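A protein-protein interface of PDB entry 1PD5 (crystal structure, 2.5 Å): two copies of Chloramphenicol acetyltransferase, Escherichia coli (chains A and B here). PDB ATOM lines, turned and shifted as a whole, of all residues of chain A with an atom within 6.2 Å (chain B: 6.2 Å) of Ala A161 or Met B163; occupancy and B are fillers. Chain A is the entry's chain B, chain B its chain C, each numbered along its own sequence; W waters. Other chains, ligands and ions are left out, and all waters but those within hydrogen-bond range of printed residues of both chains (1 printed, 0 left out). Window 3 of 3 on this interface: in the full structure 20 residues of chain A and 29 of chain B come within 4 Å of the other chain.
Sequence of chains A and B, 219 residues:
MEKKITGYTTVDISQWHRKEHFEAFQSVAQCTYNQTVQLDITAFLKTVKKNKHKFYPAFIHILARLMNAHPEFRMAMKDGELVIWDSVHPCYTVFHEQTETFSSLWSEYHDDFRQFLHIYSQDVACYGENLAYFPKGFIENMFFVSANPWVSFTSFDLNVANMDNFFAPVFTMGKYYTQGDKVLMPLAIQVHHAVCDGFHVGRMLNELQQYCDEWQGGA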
ATOM      1  N   ASN A 159      23.374  29.948  11.841  1.00  0.00           N
ATOM      2  CA  ASN A 159      21.950  29.938  11.525  1.00  0.00           C
ATOM      3  C   ASN A 159      21.611  28.466  11.106  1.00  0.00           C
ATOM      4  O   ASN A 159      21.754  27.997   9.931  1.00  0.00           O
ATOM      5  CB  ASN A 159      21.456  31.089  10.547  1.00  0.00           C
ATOM      6  CG  ASN A 159      20.059  30.697   9.679  1.00  0.00           C
ATOM      7  OD1 ASN A 159      19.938  30.964   8.395  1.00  0.00           O
ATOM      8  ND2 ASN A 159      19.012  30.168  10.387  1.00  0.00           N
ATOM      9  N   VAL A 160      21.268  27.712  12.109  1.00  0.00           N
ATOM     10  CA  VAL A 160      20.723  26.393  11.967  1.00  0.00           C
ATOM     11  C   VAL A 160      19.327  26.572  11.296  1.00  0.00           C
ATOM     12  O   VAL A 160      18.584  27.468  11.639  1.00  0.00           O
ATOM     13  CB  VAL A 160      20.717  25.864  13.350  1.00  0.00           C
ATOM     14  CG1 VAL A 160      19.518  25.417  13.837  1.00  0.00           C
ATOM     15  CG2 VAL A 160      21.961  25.080  13.675  1.00  0.00           C
ATOM     16  N   ALA A 161      19.058  25.751  10.287  1.00  0.00           N
ATOM     17  CA  ALA A 161      17.796  25.685   9.589  1.00  0.00           C
ATOM     18  C   ALA A 161      16.759  25.030  10.280  1.00  0.00           C
ATOM     19  O   ALA A 161      15.631  25.276   9.932  1.00  0.00           O
ATOM     20  CB  ALA A 161      17.984  24.839   8.295  1.00  0.00           C
ATOM     21  N   ASN A 162      17.081  24.025  11.111  1.00  0.00           N
ATOM     22  CA  ASN A 162      16.027  23.225  11.754  1.00  0.00           C
ATOM     23  C   ASN A 162      16.267  23.428  13.242  1.00  0.00           C
ATOM     24  O   ASN A 162      17.244  22.898  13.801  1.00  0.00           O
ATOM     25  CB  ASN A 162      16.111  21.757  11.286  1.00  0.00           C
ATOM     26  CG  ASN A 162      16.024  21.606   9.685  1.00  0.00           C
ATOM     27  OD1 ASN A 162      15.129  22.257   9.062  1.00  0.00           O
ATOM     28  ND2 ASN A 162      16.971  20.799   9.011  1.00  0.00           N
ATOM     29  N   MET A 163      15.418  24.220  13.917  1.00  0.00           N
ATOM     30  CA  MET A 163      15.758  24.588  15.306  1.00  0.00           C
ATOM     31  C   MET A 163      14.960  23.953  16.459  1.00  0.00           C
ATOM     32  O   MET A 163      15.244  24.226  17.666  1.00  0.00           O
ATOM     33  CB  MET A 163      15.886  26.060  15.439  1.00  0.00           C
ATOM     34  CG  MET A 163      14.624  26.734  15.571  1.00  0.00           C
ATOM     35  SD  MET A 163      14.732  28.542  15.595  1.00  0.00           S
ATOM     36  CE  MET A 163      15.497  28.808  14.174  1.00  0.00           C
ATOM     37  N   GLN B  26      23.582  18.956   4.289  1.00  0.00           N
ATOM     38  CA  GLN B  26      22.386  19.002   3.414  1.00  0.00           C
ATOM     39  C   GLN B  26      21.071  18.560   4.032  1.00  0.00           C
ATOM     40  O   GLN B  26      19.984  18.859   3.494  1.00  0.00           O
ATOM     41  CB  GLN B  26      22.631  18.210   2.111  1.00  0.00           C
ATOM     42  CG  GLN B  26      23.625  18.873   1.328  1.00  0.00           C
ATOM     43  CD  GLN B  26      23.097  20.070   0.632  1.00  0.00           C
ATOM     44  OE1 GLN B  26      22.543  19.993  -0.494  1.00  0.00           O
ATOM     45  NE2 GLN B  26      23.232  21.181   1.276  1.00  0.00           N
ATOM     46  N   VAL B  28      19.999  17.592   7.973  1.00  0.00           N
ATOM     47  CA  VAL B  28      19.275  17.808   9.260  1.00  0.00           C
ATOM     48  C   VAL B  28      19.865  18.805  10.245  1.00  0.00           C
ATOM     49  O   VAL B  28      19.213  19.821  10.607  1.00  0.00           O
ATOM     50  CB  VAL B  28      18.572  16.558   9.963  1.00  0.00           C
ATOM     51  CG1 VAL B  28      19.534  15.420  10.123  1.00  0.00           C
ATOM     52  CG2 VAL B  28      17.743  17.037  11.366  1.00  0.00           C
ATOM     53  N   ALA B  29      21.125  18.584  10.522  1.00  0.00           N
ATOM     54  CA  ALA B  29      22.071  19.650  10.664  1.00  0.00           C
ATOM     55  C   ALA B  29      22.322  20.823   9.566  1.00  0.00           C
ATOM     56  O   ALA B  29      23.260  21.640   9.704  1.00  0.00           O
ATOM     57  CB  ALA B  29      23.368  19.037  11.032  1.00  0.00           C
ATOM     58  N   GLN B  30      21.562  20.945   8.498  1.00  0.00           N
ATOM     59  CA  GLN B  30      21.855  22.053   7.587  1.00  0.00           C
ATOM     60  C   GLN B  30      22.066  23.332   8.393  1.00  0.00           C
ATOM     61  O   GLN B  30      21.429  23.547   9.407  1.00  0.00           O
ATOM     62  CB  GLN B  30      20.707  22.277   6.724  1.00  0.00           C
ATOM     63  CG  GLN B  30      21.174  23.171   5.492  1.00  0.00           C
ATOM     64  CD  GLN B  30      20.052  23.244   4.428  1.00  0.00           C
ATOM     65  OE1 GLN B  30      18.974  22.709   4.714  1.00  0.00           O
ATOM     66  NE2 GLN B  30      20.283  23.885   3.275  1.00  0.00           N
ATOM     67  N   CYS B  31      23.024  24.150   7.998  1.00  0.00           N
ATOM     68  CA  CYS B  31      23.177  25.462   8.643  1.00  0.00           C
ATOM     69  C   CYS B  31      24.026  26.330   7.815  1.00  0.00           C
ATOM     70  O   CYS B  31      24.834  25.879   7.000  1.00  0.00           O
ATOM     71  CB  CYS B  31      23.741  25.384  10.040  1.00  0.00           C
ATOM     72  SG  CYS B  31      25.323  24.632  10.051  1.00  0.00           S
ATOM     73  N   THR B  32      23.888  27.591   8.070  1.00  0.00           N
ATOM     74  CA  THR B  32      24.659  28.662   7.473  1.00  0.00           C
ATOM     75  C   THR B  32      25.416  29.324   8.630  1.00  0.00           C
ATOM     76  O   THR B  32      25.139  29.160   9.895  1.00  0.00           O
ATOM     77  CB  THR B  32      23.520  29.466   6.928  1.00  0.00           C
ATOM     78  OG1 THR B  32      23.429  29.382   5.466  1.00  0.00           O
ATOM     79  CG2 THR B  32      23.398  30.804   7.292  1.00  0.00           C
ATOM     80  N   ASN B 159      20.556  36.264   7.494  1.00  0.00           N
ATOM     81  CA  ASN B 159      19.763  35.123   7.859  1.00  0.00           C
ATOM     82  C   ASN B 159      18.709  34.907   6.742  1.00  0.00           C
ATOM     83  O   ASN B 159      17.638  35.634   6.574  1.00  0.00           O
ATOM     84  CB  ASN B 159      19.177  35.251   9.264  1.00  0.00           C
ATOM     85  CG  ASN B 159      18.097  34.129   9.634  1.00  0.00           C
ATOM     86  OD1 ASN B 159      17.044  34.464  10.286  1.00  0.00           O
ATOM     87  ND2 ASN B 159      18.329  32.807   9.239  1.00  0.00           N
ATOM     88  N   VAL B 160      19.030  33.898   5.960  1.00  0.00           N
ATOM     89  CA  VAL B 160      18.281  33.540   4.745  1.00  0.00           C
ATOM     90  C   VAL B 160      17.200  32.624   5.291  1.00  0.00           C
ATOM     91  O   VAL B 160      17.447  31.645   5.979  1.00  0.00           O
ATOM     92  CB  VAL B 160      19.320  32.894   3.842  1.00  0.00           C
ATOM     93  CG1 VAL B 160      18.902  31.640   3.264  1.00  0.00           C
ATOM     94  CG2 VAL B 160      19.924  33.895   2.925  1.00  0.00           C
ATOM     95  N   ALA B 161      15.952  32.954   5.016  1.00  0.00           N
ATOM     96  CA  ALA B 161      14.896  31.982   5.281  1.00  0.00           C
ATOM     97  C   ALA B 161      15.108  30.676   4.650  1.00  0.00           C
ATOM     98  O   ALA B 161      14.591  29.706   5.096  1.00  0.00           O
ATOM     99  CB  ALA B 161      13.648  32.449   4.815  1.00  0.00           C
ATOM    100  N   ASN B 162      15.782  30.610   3.541  1.00  0.00           N
ATOM    101  CA  ASN B 162      15.776  29.319   2.809  1.00  0.00           C
ATOM    102  C   ASN B 162      17.128  28.975   2.333  1.00  0.00           C
ATOM    103  O   ASN B 162      17.580  29.591   1.290  1.00  0.00           O
ATOM    104  CB  ASN B 162      15.156  29.557   1.520  1.00  0.00           C
ATOM    105  CG  ASN B 162      14.090  28.777   1.336  1.00  0.00           C
ATOM    106  OD1 ASN B 162      14.164  27.639   0.632  1.00  0.00           O
ATOM    107  ND2 ASN B 162      12.972  29.279   1.926  1.00  0.00           N
ATOM    108  N   MET B 163      17.749  28.044   3.035  1.00  0.00           N
ATOM    109  CA  MET B 163      19.142  27.831   2.768  1.00  0.00           C
ATOM    110  C   MET B 163      19.393  26.612   1.900  1.00  0.00           C
ATOM    111  O   MET B 163      20.589  26.256   1.714  1.00  0.00           O
ATOM    112  CB  MET B 163      19.978  27.712   4.073  1.00  0.00           C
ATOM    113  CG  MET B 163      19.437  26.764   5.104  1.00  0.00           C
ATOM    114  SD  MET B 163      20.571  26.810   6.483  1.00  0.00           S
ATOM    115  CE  MET B 163      19.730  28.085   7.272  1.00  0.00           C
ATOM    116  N   ASP B 164      18.351  25.967   1.390  1.00  0.00           N
ATOM    117  CA  ASP B 164      18.600  24.871   0.444  1.00  0.00           C
ATOM    118  C   ASP B 164      19.497  25.282  -0.698  1.00  0.00           C
ATOM    119  O   ASP B 164      19.238  26.223  -1.363  1.00  0.00           O
ATOM    120  CB  ASP B 164      17.326  24.177  -0.092  1.00  0.00           C
ATOM    121  CG  ASP B 164      16.568  23.571   0.991  1.00  0.00           C
ATOM    122  OD1 ASP B 164      17.140  23.207   2.092  1.00  0.00           O
ATOM    123  OD2 ASP B 164      15.378  23.454   0.916  1.00  0.00           O
ATOM    124  N   ASN B 165      20.558  24.512  -0.916  1.00  0.00           N
ATOM    125  CA  ASN B 165      21.529  24.693  -1.990  1.00  0.00           C
ATOM    126  C   ASN B 165      22.100  26.130  -2.129  1.00  0.00           C
ATOM    127  O   ASN B 165      22.700  26.463  -3.175  1.00  0.00           O
ATOM    128  CB  ASN B 165      20.836  24.215  -3.250  1.00  0.00           C
ATOM    129  CG  ASN B 165      20.267  22.753  -3.087  1.00  0.00           C
ATOM    130  OD1 ASN B 165      20.866  21.914  -2.435  1.00  0.00           O
ATOM    131  ND2 ASN B 165      19.145  22.482  -3.692  1.00  0.00           N
ATOM    132  N   PHE B 166      21.908  26.993  -1.118  1.00  0.00           N
ATOM    133  CA  PHE B 166      22.373  28.321  -1.278  1.00  0.00           C
ATOM    134  C   PHE B 166      23.882  28.398  -0.911  1.00  0.00           C
ATOM    135  O   PHE B 166      24.249  28.540   0.277  1.00  0.00           O
ATOM    136  CB  PHE B 166      21.595  29.192  -0.369  1.00  0.00           C
ATOM    137  CG  PHE B 166      22.038  30.632  -0.453  1.00  0.00           C
ATOM    138  CD1 PHE B 166      22.134  31.283  -1.717  1.00  0.00           C
ATOM    139  CD2 PHE B 166      22.494  31.296   0.656  1.00  0.00           C
ATOM    140  CE1 PHE B 166      22.575  32.526  -1.845  1.00  0.00           C
ATOM    141  CE2 PHE B 166      22.906  32.607   0.519  1.00  0.00           C
ATOM    142  CZ  PHE B 166      22.962  33.239  -0.692  1.00  0.00           C
ATOM    143  N   PHE B 167      24.749  28.286  -1.931  1.00  0.00           N
ATOM    144  CA  PHE B 167      26.086  27.881  -1.740  1.00  0.00           C
ATOM    145  C   PHE B 167      26.947  29.026  -2.113  1.00  0.00           C
ATOM    146  O   PHE B 167      28.135  28.992  -1.908  1.00  0.00           O
ATOM    147  CB  PHE B 167      26.417  26.663  -2.707  1.00  0.00           C
ATOM    148  CG  PHE B 167      25.846  25.313  -2.227  1.00  0.00           C
ATOM    149  CD1 PHE B 167      25.309  25.202  -0.904  1.00  0.00           C
ATOM    150  CD2 PHE B 167      25.843  24.189  -3.066  1.00  0.00           C
ATOM    151  CE1 PHE B 167      24.770  24.012  -0.445  1.00  0.00           C
ATOM    152  CE2 PHE B 167      25.399  22.989  -2.613  1.00  0.00           C
ATOM    153  CZ  PHE B 167      24.795  22.863  -1.328  1.00  0.00           C
ATOM    154  N   HIS B 192      27.669  28.515   3.427  1.00  0.00           N
ATOM    155  CA  HIS B 192      26.787  27.467   3.790  1.00  0.00           C
ATOM    156  C   HIS B 192      27.705  26.321   4.194  1.00  0.00           C
ATOM    157  O   HIS B 192      28.723  26.052   3.547  1.00  0.00           O
ATOM    158  CB  HIS B 192      26.070  27.044   2.588  1.00  0.00           C
ATOM    159  CG  HIS B 192      24.935  26.116   2.827  1.00  0.00           C
ATOM    160  ND1 HIS B 192      25.121  24.783   3.157  1.00  0.00           N
ATOM    161  CD2 HIS B 192      23.589  26.310   2.710  1.00  0.00           C
ATOM    162  CE1 HIS B 192      23.915  24.189   3.254  1.00  0.00           C
ATOM    163  NE2 HIS B 192      22.985  25.088   2.986  1.00  0.00           N
HETATM  164  O   HOH W   1      17.398  20.784   6.311  1.00  0.00           O
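The backbone carbonyl oxygen (O) of Thr B32 lies within hydrogen-bond range of the backbone NH (N) of Asn A159 (2.7 Å). The backbone carbonyl oxygen of Gln B30 lies within hydrogen-bond range of the backbone NH of Ala A161, at 3.4 Å. The side-chain amide nitrogen (ND2) of Asn B159 is in hydrogen-bond range of the side-chain amide oxygen (OD1) of Asn A159 (2.6 Å). O of Val B28 sits at hydrogen-bond distance from ND2 of Asn A162 (2.9 Å).
The side-chain sulfur (SG) of Cys B31 lies within hydrogen-bond range of the backbone carbonyl oxygen (O) of Ala B29. SD of Met B163 sits at hydrogen-bond distance from N of Thr B32 (3.8 Å). OE1 of Gln B30 lies close to OD1 of Asp B164 (3.2 Å). The side-chain amide nitrogen (NE2) of Gln B30 sits at hydrogen-bond distance from a ring nitrogen (NE2) of His B192 (3.0 Å). The backbone carbonyl oxygen of Met B163 is in hydrogen-bond range of a ring nitrogen (NE2) of His B192. The side-chain amide nitrogen of Gln B30 lies within hydrogen-bond range of the backbone carbonyl oxygen of Met B163 (2.9 Å).
CA of Cys B31 touches O of Asn A159 (3.2 Å). Val B160 touches Asn A159 (O to OD1, 3.5 Å). Asn A159 touches Met B163 (OD1 to CE, 3.1 Å). Val A160 touches Gln B30. Val A160 touches Cys B31 (CA to CB, 3.7 Å). Ala A161 touches Met B163.
Ala A161 touches just these residues of chain B: Gln B30 and Met B163. Of the printed residues of chain A, Cys B31 touches Asn A159 (3.2 Å) and Val A160 (3.7 Å). Of the printed residues of chain A, Thr B32 touches Asn A159 (2.7 Å). Of the printed residues of chain A, Asn B159 touches Asn A159. Of chain A, only Asn A159 (3.1 Å) and Ala A161 (3.7 Å) come within 4 Å of Met B163. Asp B164 touches none of the printed residues of chain A. His B192 touches none of the printed residues of chain A. The nearest printed residue of chain B that does not touch Val A160 is Met B163 (4.3 Å).
Hydrophobic or aromatic side chains of chain B that line the printed part of chain A: Met B163. Of the 5 printed residues of chain A, 4 touch a printed residue of chain B. Among the printed residues, 10 pairs touch across the chains. Among the printed residues, no Asp or Glu carboxylate lies within 4 Å of a Lys or Arg side-chain nitrogen of the other chain.
Asn B159 touches its own counterpart, Asn A159. Asn A159 touches Val B160, but with the chains exchanged Val A160 does not touch Asn B159 (5.9 Å). Asn A159 touches Met B163, but with the chains exchanged Met A163 does not touch Asn B159 (7.0 Å). Ala A161 touches Met B163, but with the chains exchanged Met A163 does not touch Ala B161 (9.2 Å).
Water W1 bridges the side-chain amide nitrogen of Asn A162 (2.7 Å) and the side-chain amide oxygen of Gln B30 (3.0 Å).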
